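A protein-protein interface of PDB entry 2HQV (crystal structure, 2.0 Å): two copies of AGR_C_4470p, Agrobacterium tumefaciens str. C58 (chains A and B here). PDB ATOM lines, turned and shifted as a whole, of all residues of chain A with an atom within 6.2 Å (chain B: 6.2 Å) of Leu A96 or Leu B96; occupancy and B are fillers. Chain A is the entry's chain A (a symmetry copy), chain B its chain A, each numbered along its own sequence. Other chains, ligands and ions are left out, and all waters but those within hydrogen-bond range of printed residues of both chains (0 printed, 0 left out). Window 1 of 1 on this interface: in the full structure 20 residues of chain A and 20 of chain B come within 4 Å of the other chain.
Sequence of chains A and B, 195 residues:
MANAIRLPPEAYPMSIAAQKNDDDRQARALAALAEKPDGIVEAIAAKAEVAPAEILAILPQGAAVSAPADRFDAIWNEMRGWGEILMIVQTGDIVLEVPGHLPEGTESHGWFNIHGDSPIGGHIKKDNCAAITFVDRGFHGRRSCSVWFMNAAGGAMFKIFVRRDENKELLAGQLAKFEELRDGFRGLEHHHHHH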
ATOM      1  N   MET A  87      18.321  -4.640  31.652  1.00  0.00           N
ATOM      2  CA  MET A  87      19.462  -5.044  30.850  1.00  0.00           C
ATOM      3  C   MET A  87      20.708  -4.349  31.382  1.00  0.00           C
ATOM      4  O   MET A  87      20.704  -3.138  31.598  1.00  0.00           O
ATOM      5  CB  MET A  87      19.235  -4.663  29.381  1.00  0.00           C
ATOM      6  CG  MET A  87      20.522  -4.463  28.591  1.00  0.00           C
ATOM      7  SD  MET A  87      21.518  -6.074  28.091  1.00  0.00           S
ATOM      8  CE  MET A  87      21.566  -7.054  29.690  1.00  0.00           C
ATOM      9  N   ILE A  88      21.772  -5.110  31.611  1.00  0.00           N
ATOM     10  CA  ILE A  88      23.004  -4.513  32.114  1.00  0.00           C
ATOM     11  C   ILE A  88      24.254  -4.952  31.355  1.00  0.00           C
ATOM     12  O   ILE A  88      24.501  -6.140  31.162  1.00  0.00           O
ATOM     13  CB  ILE A  88      23.230  -4.832  33.604  1.00  0.00           C
ATOM     14  CG1 ILE A  88      22.046  -4.336  34.434  1.00  0.00           C
ATOM     15  CG2 ILE A  88      24.518  -4.151  34.092  1.00  0.00           C
ATOM     16  CD1 ILE A  88      22.215  -4.561  35.928  1.00  0.00           C
ATOM     17  N   VAL A  89      25.030  -3.968  30.922  1.00  0.00           N
ATOM     18  CA  VAL A  89      26.278  -4.208  30.216  1.00  0.00           C
ATOM     19  C   VAL A  89      27.296  -3.477  31.072  1.00  0.00           C
ATOM     20  O   VAL A  89      27.050  -2.345  31.491  1.00  0.00           O
ATOM     21  CB  VAL A  89      26.275  -3.601  28.795  1.00  0.00           C
ATOM     22  CG1 VAL A  89      27.699  -3.596  28.220  1.00  0.00           C
ATOM     23  CG2 VAL A  89      25.359  -4.418  27.879  1.00  0.00           C
ATOM     24  N   GLN A  90      28.426  -4.119  31.339  1.00  0.00           N
ATOM     25  CA  GLN A  90      29.459  -3.516  32.173  1.00  0.00           C
ATOM     26  C   GLN A  90      30.874  -3.697  31.635  1.00  0.00           C
ATOM     27  O   GLN A  90      31.234  -4.765  31.151  1.00  0.00           O
ATOM     28  CB  GLN A  90      29.366  -4.089  33.597  1.00  0.00           C
ATOM     29  CG  GLN A  90      30.632  -3.925  34.439  1.00  0.00           C
ATOM     30  CD  GLN A  90      30.403  -4.246  35.906  1.00  0.00           C
ATOM     31  OE1 GLN A  90      29.547  -5.060  36.248  1.00  0.00           O
ATOM     32  NE2 GLN A  90      31.182  -3.614  36.781  1.00  0.00           N
ATOM     33  N   ILE A  94      32.304   1.654  32.429  1.00  0.00           N
ATOM     34  CA  ILE A  94      30.889   1.972  32.572  1.00  0.00           C
ATOM     35  C   ILE A  94      29.974   0.780  32.824  1.00  0.00           C
ATOM     36  O   ILE A  94      30.224  -0.329  32.342  1.00  0.00           O
ATOM     37  CB  ILE A  94      30.377   2.699  31.295  1.00  0.00           C
ATOM     38  CG1 ILE A  94      28.929   3.171  31.472  1.00  0.00           C
ATOM     39  CG2 ILE A  94      30.443   1.746  30.099  1.00  0.00           C
ATOM     40  CD1 ILE A  94      28.405   3.994  30.282  1.00  0.00           C
ATOM     41  N   VAL A  95      28.919   1.032  33.593  1.00  0.00           N
ATOM     42  CA  VAL A  95      27.891   0.041  33.878  1.00  0.00           C
ATOM     43  C   VAL A  95      26.606   0.698  33.360  1.00  0.00           C
ATOM     44  O   VAL A  95      26.133   1.690  33.922  1.00  0.00           O
ATOM     45  CB  VAL A  95      27.717  -0.234  35.390  1.00  0.00           C
ATOM     46  CG1 VAL A  95      26.573  -1.225  35.593  1.00  0.00           C
ATOM     47  CG2 VAL A  95      29.008  -0.792  35.986  1.00  0.00           C
ATOM     48  N   LEU A  96      26.065   0.177  32.267  1.00  0.00           N
ATOM     49  CA  LEU A  96      24.849   0.740  31.697  1.00  0.00           C
ATOM     50  C   LEU A  96      23.665  -0.148  32.066  1.00  0.00           C
ATOM     51  O   LEU A  96      23.645  -1.345  31.761  1.00  0.00           O
ATOM     52  CB  LEU A  96      24.996   0.860  30.175  1.00  0.00           C
ATOM     53  CG  LEU A  96      23.880   1.508  29.352  1.00  0.00           C
ATOM     54  CD1 LEU A  96      23.613   2.929  29.833  1.00  0.00           C
ATOM     55  CD2 LEU A  96      24.282   1.507  27.883  1.00  0.00           C
ATOM     56  N   GLU A  97      22.686   0.445  32.738  1.00  0.00           N
ATOM     57  CA  GLU A  97      21.494  -0.281  33.171  1.00  0.00           C
ATOM     58  C   GLU A  97      20.296   0.318  32.457  1.00  0.00           C
ATOM     59  O   GLU A  97      19.989   1.496  32.619  1.00  0.00           O
ATOM     60  CB  GLU A  97      21.344  -0.164  34.689  1.00  0.00           C
ATOM     61  CG  GLU A  97      22.596  -0.611  35.426  1.00  0.00           C
ATOM     62  CD  GLU A  97      22.558  -0.322  36.915  1.00  0.00           C
ATOM     63  OE1 GLU A  97      23.562  -0.614  37.592  1.00  0.00           O
ATOM     64  OE2 GLU A  97      21.531   0.189  37.410  1.00  0.00           O
ATOM     65  N   VAL A  98      19.631  -0.510  31.660  1.00  0.00           N
ATOM     66  CA  VAL A  98      18.489  -0.078  30.873  1.00  0.00           C
ATOM     67  C   VAL A  98      17.248  -0.917  31.135  1.00  0.00           C
ATOM     68  O   VAL A  98      17.241  -2.125  30.901  1.00  0.00           O
ATOM     69  CB  VAL A  98      18.805  -0.159  29.358  1.00  0.00           C
ATOM     70  CG1 VAL A  98      17.692   0.518  28.543  1.00  0.00           C
ATOM     71  CG2 VAL A  98      20.168   0.481  29.071  1.00  0.00           C
ATOM     72  N   ILE A 114      18.966  -6.606  17.599  1.00  0.00           N
ATOM     73  CA  ILE A 114      17.727  -6.352  18.321  1.00  0.00           C
ATOM     74  C   ILE A 114      17.228  -4.918  18.222  1.00  0.00           C
ATOM     75  O   ILE A 114      17.926  -3.972  18.593  1.00  0.00           O
ATOM     76  CB  ILE A 114      17.883  -6.707  19.811  1.00  0.00           C
ATOM     77  CG1 ILE A 114      19.129  -6.019  20.384  1.00  0.00           C
ATOM     78  CG2 ILE A 114      17.956  -8.220  19.977  1.00  0.00           C
ATOM     79  CD1 ILE A 114      19.294  -6.196  21.889  1.00  0.00           C
ATOM     80  N   PRO A 119      13.696   0.788  24.655  1.00  0.00           N
ATOM     81  CA  PRO A 119      14.949   1.545  24.644  1.00  0.00           C
ATOM     82  C   PRO A 119      16.154   0.607  24.563  1.00  0.00           C
ATOM     83  O   PRO A 119      17.273   1.047  24.316  1.00  0.00           O
ATOM     84  CB  PRO A 119      14.897   2.317  25.958  1.00  0.00           C
ATOM     85  CG  PRO A 119      14.110   1.407  26.857  1.00  0.00           C
ATOM     86  CD  PRO A 119      12.993   0.947  25.939  1.00  0.00           C
ATOM     87  N   ILE A 120      15.917  -0.682  24.777  1.00  0.00           N
ATOM     88  CA  ILE A 120      16.988  -1.677  24.704  1.00  0.00           C
ATOM     89  C   ILE A 120      17.145  -2.061  23.239  1.00  0.00           C
ATOM     90  O   ILE A 120      16.282  -2.725  22.674  1.00  0.00           O
ATOM     91  CB  ILE A 120      16.644  -2.952  25.510  1.00  0.00           C
ATOM     92  CG1 ILE A 120      16.548  -2.620  26.998  1.00  0.00           C
ATOM     93  CG2 ILE A 120      17.714  -4.036  25.272  1.00  0.00           C
ATOM     94  CD1 ILE A 120      16.108  -3.795  27.855  1.00  0.00           C
ATOM     95  N   GLY A 121      18.240  -1.635  22.624  1.00  0.00           N
ATOM     96  CA  GLY A 121      18.472  -1.963  21.231  1.00  0.00           C
ATOM     97  C   GLY A 121      19.949  -2.087  20.911  1.00  0.00           C
ATOM     98  O   GLY A 121      20.808  -1.789  21.743  1.00  0.00           O
ATOM     99  N   GLY A 122      20.250  -2.527  19.698  1.00  0.00           N
ATOM    100  CA  GLY A 122      21.636  -2.674  19.313  1.00  0.00           C
ATOM    101  C   GLY A 122      21.968  -3.995  18.663  1.00  0.00           C
ATOM    102  O   GLY A 122      21.178  -4.537  17.883  1.00  0.00           O
ATOM    103  N   HIS A 123      23.136  -4.531  19.015  1.00  0.00           N
ATOM    104  CA  HIS A 123      23.615  -5.767  18.410  1.00  0.00           C
ATOM    105  C   HIS A 123      24.369  -6.657  19.376  1.00  0.00           C
ATOM    106  O   HIS A 123      25.313  -6.210  20.032  1.00  0.00           O
ATOM    107  CB  HIS A 123      24.540  -5.413  17.250  1.00  0.00           C
ATOM    108  CG  HIS A 123      24.001  -4.335  16.369  1.00  0.00           C
ATOM    109  ND1 HIS A 123      23.143  -4.588  15.322  1.00  0.00           N
ATOM    110  CD2 HIS A 123      24.148  -2.989  16.421  1.00  0.00           C
ATOM    111  CE1 HIS A 123      22.780  -3.445  14.768  1.00  0.00           C
ATOM    112  NE2 HIS A 123      23.376  -2.459  15.417  1.00  0.00           N
ATOM    113  N   MET B  87      22.665   6.930  23.338  1.00  0.00           N
ATOM    114  CA  MET B  87      23.793   6.476  24.132  1.00  0.00           C
ATOM    115  C   MET B  87      24.264   5.132  23.593  1.00  0.00           C
ATOM    116  O   MET B  87      23.459   4.227  23.380  1.00  0.00           O
ATOM    117  CB  MET B  87      23.380   6.337  25.603  1.00  0.00           C
ATOM    118  CG  MET B  87      24.217   5.334  26.386  1.00  0.00           C
ATOM    119  SD  MET B  87      26.033   5.882  26.875  1.00  0.00           S
ATOM    120  CE  MET B  87      26.707   6.589  25.274  1.00  0.00           C
ATOM    121  N   ILE B  88      25.564   5.000  23.356  1.00  0.00           N
ATOM    122  CA  ILE B  88      26.090   3.738  22.847  1.00  0.00           C
ATOM    123  C   ILE B  88      27.323   3.238  23.597  1.00  0.00           C
ATOM    124  O   ILE B  88      28.295   3.966  23.786  1.00  0.00           O
ATOM    125  CB  ILE B  88      26.461   3.832  21.354  1.00  0.00           C
ATOM    126  CG1 ILE B  88      25.240   4.245  20.533  1.00  0.00           C
ATOM    127  CG2 ILE B  88      26.974   2.470  20.860  1.00  0.00           C
ATOM    128  CD1 ILE B  88      25.506   4.305  19.037  1.00  0.00           C
ATOM    129  N   VAL B  89      27.256   1.987  24.027  1.00  0.00           N
ATOM    130  CA  VAL B  89      28.355   1.339  24.725  1.00  0.00           C
ATOM    131  C   VAL B  89      28.630   0.119  23.864  1.00  0.00           C
ATOM    132  O   VAL B  89      27.694  -0.566  23.450  1.00  0.00           O
ATOM    133  CB  VAL B  89      27.960   0.882  26.148  1.00  0.00           C
ATOM    134  CG1 VAL B  89      29.028  -0.064  26.714  1.00  0.00           C
ATOM    135  CG2 VAL B  89      27.819   2.099  27.068  1.00  0.00           C
ATOM    136  N   GLN B  90      29.901  -0.146  23.589  1.00  0.00           N
ATOM    137  CA  GLN B  90      30.271  -1.279  22.750  1.00  0.00           C
ATOM    138  C   GLN B  90      31.455  -2.081  23.279  1.00  0.00           C
ATOM    139  O   GLN B  90      32.435  -1.519  23.758  1.00  0.00           O
ATOM    140  CB  GLN B  90      30.571  -0.785  21.325  1.00  0.00           C
ATOM    141  CG  GLN B  90      31.407  -1.743  20.476  1.00  0.00           C
ATOM    142  CD  GLN B  90      31.439  -1.348  19.009  1.00  0.00           C
ATOM    143  OE1 GLN B  90      31.333  -0.170  18.671  1.00  0.00           O
ATOM    144  NE2 GLN B  90      31.599  -2.335  18.131  1.00  0.00           N
ATOM    145  N   ILE B  94      28.983  -7.038  22.489  1.00  0.00           N
ATOM    146  CA  ILE B  94      27.711  -6.340  22.355  1.00  0.00           C
ATOM    147  C   ILE B  94      27.812  -4.840  22.106  1.00  0.00           C
ATOM    148  O   ILE B  94      28.735  -4.175  22.583  1.00  0.00           O
ATOM    149  CB  ILE B  94      26.853  -6.550  23.636  1.00  0.00           C
ATOM    150  CG1 ILE B  94      25.454  -5.945  23.470  1.00  0.00           C
ATOM    151  CG2 ILE B  94      27.541  -5.882  24.830  1.00  0.00           C
ATOM    152  CD1 ILE B  94      24.524  -6.219  24.665  1.00  0.00           C
ATOM    153  N   VAL B  95      26.849  -4.329  21.344  1.00  0.00           N
ATOM    154  CA  VAL B  95      26.731  -2.906  21.063  1.00  0.00           C
ATOM    155  C   VAL B  95      25.336  -2.549  21.591  1.00  0.00           C
ATOM    156  O   VAL B  95      24.323  -2.979  21.034  1.00  0.00           O
ATOM    157  CB  VAL B  95      26.773  -2.581  19.551  1.00  0.00           C
ATOM    158  CG1 VAL B  95      26.570  -1.080  19.354  1.00  0.00           C
ATOM    159  CG2 VAL B  95      28.107  -3.015  18.946  1.00  0.00           C
ATOM    160  N   LEU B  96      25.282  -1.803  22.685  1.00  0.00           N
ATOM    161  CA  LEU B  96      24.002  -1.423  23.265  1.00  0.00           C
ATOM    162  C   LEU B  96      23.699   0.027  22.901  1.00  0.00           C
ATOM    163  O   LEU B  96      24.477   0.937  23.203  1.00  0.00           O
ATOM    164  CB  LEU B  96      24.042  -1.614  24.786  1.00  0.00           C
ATOM    165  CG  LEU B  96      22.782  -1.363  25.617  1.00  0.00           C
ATOM    166  CD1 LEU B  96      21.638  -2.252  25.142  1.00  0.00           C
ATOM    167  CD2 LEU B  96      23.093  -1.632  27.084  1.00  0.00           C
ATOM    168  N   GLU B  97      22.568   0.232  22.236  1.00  0.00           N
ATOM    169  CA  GLU B  97      22.152   1.566  21.809  1.00  0.00           C
ATOM    170  C   GLU B  97      20.862   1.907  22.532  1.00  0.00           C
ATOM    171  O   GLU B  97      19.851   1.227  22.375  1.00  0.00           O
ATOM    172  CB  GLU B  97      21.952   1.581  20.293  1.00  0.00           C
ATOM    173  CG  GLU B  97      23.183   1.089  19.547  1.00  0.00           C
ATOM    174  CD  GLU B  97      22.954   0.901  18.058  1.00  0.00           C
ATOM    175  OE1 GLU B  97      23.895   0.458  17.375  1.00  0.00           O
ATOM    176  OE2 GLU B  97      21.842   1.198  17.571  1.00  0.00           O
ATOM    177  N   VAL B  98      20.916   2.966  23.331  1.00  0.00           N
ATOM    178  CA  VAL B  98      19.778   3.395  24.127  1.00  0.00           C
ATOM    179  C   VAL B  98      19.400   4.846  23.870  1.00  0.00           C
ATOM    180  O   VAL B  98      20.196   5.756  24.101  1.00  0.00           O
ATOM    181  CB  VAL B  98      20.078   3.244  25.639  1.00  0.00           C
ATOM    182  CG1 VAL B  98      18.801   3.470  26.462  1.00  0.00           C
ATOM    183  CG2 VAL B  98      20.678   1.862  25.919  1.00  0.00           C
ATOM    184  N   ILE B 114      24.536   7.945  37.381  1.00  0.00           N
ATOM    185  CA  ILE B 114      23.435   8.575  36.668  1.00  0.00           C
ATOM    186  C   ILE B 114      22.112   7.830  36.773  1.00  0.00           C
ATOM    187  O   ILE B 114      22.007   6.659  36.401  1.00  0.00           O
ATOM    188  CB  ILE B 114      23.777   8.742  35.176  1.00  0.00           C
ATOM    189  CG1 ILE B 114      24.253   7.403  34.597  1.00  0.00           C
ATOM    190  CG2 ILE B 114      24.832   9.829  35.006  1.00  0.00           C
ATOM    191  CD1 ILE B 114      24.485   7.430  33.090  1.00  0.00           C
ATOM    192  N   PRO B 119      15.650   5.902  30.376  1.00  0.00           N
ATOM    193  CA  PRO B 119      16.088   4.505  30.381  1.00  0.00           C
ATOM    194  C   PRO B 119      17.613   4.412  30.452  1.00  0.00           C
ATOM    195  O   PRO B 119      18.163   3.341  30.693  1.00  0.00           O
ATOM    196  CB  PRO B 119      15.530   3.964  29.069  1.00  0.00           C
ATOM    197  CG  PRO B 119      15.537   5.169  28.173  1.00  0.00           C
ATOM    198  CD  PRO B 119      15.009   6.250  29.097  1.00  0.00           C
ATOM    199  N   ILE B 120      18.287   5.536  30.237  1.00  0.00           N
ATOM    200  CA  ILE B 120      19.748   5.573  30.301  1.00  0.00           C
ATOM    201  C   ILE B 120      20.129   5.754  31.764  1.00  0.00           C
ATOM    202  O   ILE B 120      19.924   6.821  32.332  1.00  0.00           O
ATOM    203  CB  ILE B 120      20.329   6.759  29.494  1.00  0.00           C
ATOM    204  CG1 ILE B 120      20.028   6.577  28.008  1.00  0.00           C
ATOM    205  CG2 ILE B 120      21.850   6.863  29.723  1.00  0.00           C
ATOM    206  CD1 ILE B 120      20.470   7.751  27.151  1.00  0.00           C
ATOM    207  N   GLY B 121      20.673   4.709  32.373  1.00  0.00           N
ATOM    208  CA  GLY B 121      21.072   4.798  33.764  1.00  0.00           C
ATOM    209  C   GLY B 121      22.264   3.913  34.075  1.00  0.00           C
ATOM    210  O   GLY B 121      22.706   3.124  33.238  1.00  0.00           O
ATOM    211  N   GLY B 122      22.788   4.041  35.284  1.00  0.00           N
ATOM    212  CA  GLY B 122      23.928   3.234  35.661  1.00  0.00           C
ATOM    213  C   GLY B 122      25.055   4.003  36.305  1.00  0.00           C
ATOM    214  O   GLY B 122      24.825   4.931  37.089  1.00  0.00           O
ATOM    215  N   HIS B 123      26.282   3.633  35.945  1.00  0.00           N
ATOM    216  CA  HIS B 123      27.463   4.242  36.544  1.00  0.00           C
ATOM    217  C   HIS B 123      28.611   4.413  35.571  1.00  0.00           C
ATOM    218  O   HIS B 123      29.019   3.455  34.910  1.00  0.00           O
ATOM    219  CB  HIS B 123      27.930   3.363  37.698  1.00  0.00           C
ATOM    220  CG  HIS B 123      26.818   2.908  38.586  1.00  0.00           C
ATOM    221  ND1 HIS B 123      26.348   3.663  39.637  1.00  0.00           N
ATOM    222  CD2 HIS B 123      26.037   1.801  38.536  1.00  0.00           C
ATOM    223  CE1 HIS B 123      25.323   3.044  40.197  1.00  0.00           C
ATOM    224  NE2 HIS B 123      25.114   1.913  39.545  1.00  0.00           N
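The backbone carbonyl oxygen (O) of Gly B121 lies within hydrogen-bond range of the backbone NH (N) of Glu A97 (2.7 Å).
The backbone NH of Glu B97 sits at hydrogen-bond distance from the backbone carbonyl oxygen of Gly A121 (2.7 Å).
The backbone carbonyl oxygen (O) of Pro B119 sits close to the backbone carbonyl oxygen (O) of Glu A97 (3.2 Å).
The backbone carbonyl oxygen (O) of Pro A119 lies close to the backbone carbonyl oxygen (O) of Glu B97 (3.2 Å).
The backbone carbonyl oxygen (O) of His A123 is in hydrogen-bond range of the backbone NH (N) of Val B95, 2.8 Å away.
O of His B123 is in hydrogen-bond range of N of Val A95, 2.8 Å away.
The backbone NH (N) of Leu A96 sits at hydrogen-bond distance from the backbone carbonyl oxygen (O) of Val A89, 2.8 Å away.
The backbone carbonyl oxygen (O) of Val B98 lies within hydrogen-bond range of the backbone NH (N) of Met B87 (2.8 Å).
The backbone carbonyl oxygen (O) of Ile A114 sits at hydrogen-bond distance from the backbone NH (N) of Gly A122, 3.0 Å away.
The backbone NH of Gly B122 lies within hydrogen-bond range of the backbone carbonyl oxygen of Ile B114 (3.0 Å).
N of Met A87 is in hydrogen-bond range of O of Val A98 (2.8 Å).
The backbone NH of Leu B96 is in hydrogen-bond range of the backbone carbonyl oxygen of Val B89 (2.8 Å).
Val A89 touches Leu B96.
CA of Ile A94 touches O of His B123 (3.3 Å).
Val A95 touches Gly B121 (O to O, 3.8 Å).
CG2 of Val B89 touches CD2 of Leu A96, 3.7 Å away.
Leu A96 touches Leu B96 (CD2 to CD2, 3.5 Å).
CD1 of Leu A96 touches O of Gly B121, at 3.5 Å.
Pro B119 touches Val A98 (O to CA, 3.4 Å).
Pro A119 touches Val B98.
Val B95 touches Gly A121 (O to O, 3.8 Å).
His A123 touches Ile B94 (O to CA, 3.3 Å).
Of chain B, only Val B89 (3.7 Å), Leu B96 (3.5 Å) and Gly B121 (3.5 Å) come within 4 Å of Leu A96.
Leu B96 touches three residues of chain A.
Of the printed residues of chain B, Gly A121 touches Val B95, Leu B96 and Glu B97.
Printed residues of chain B within 4 Å of His A123: Ile B94 (3.3 Å), Val B95 (2.8 Å) and Glu B97 (3.6 Å).
Of the printed residues of chain B, Ile A94 touches Val B89 (3.8 Å) and His B123 (3.3 Å).
Printed residues of chain A within 4 Å of Gly B122: Val A95 (3.2 Å).
Printed residues of chain A within 4 Å of Glu B97: Pro A119, Gly A121 and His A123.
The nearest printed residue of chain B that does not touch Leu A96 is Met B87 (4.1 Å).
The nearest printed residue of chain A that does not touch Leu B96 is Met A87 (4.1 Å).
The nearest printed residue of chain A that does not touch His B123 is Leu A96 (5.1 Å).
Among the printed residues, no Asp or Glu carboxylate lies within 4 Å of a Lys or Arg side-chain nitrogen of the other chain.
Val A95 touches Gly B122, and with the chains exchanged Gly A122 touches Val B95.
Glu A97 touches Pro B119, and with the chains exchanged Pro A119 touches Glu B97.
Glu A97 touches His B123, and with the chains exchanged His A123 touches Glu B97.
Val A98 touches its own counterpart, Val B98.
15 positions are printed for both chains.
Of the 25 pairs that touch across the chains among the printed residues, 25 have their exchanged pair printed and touching as well.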
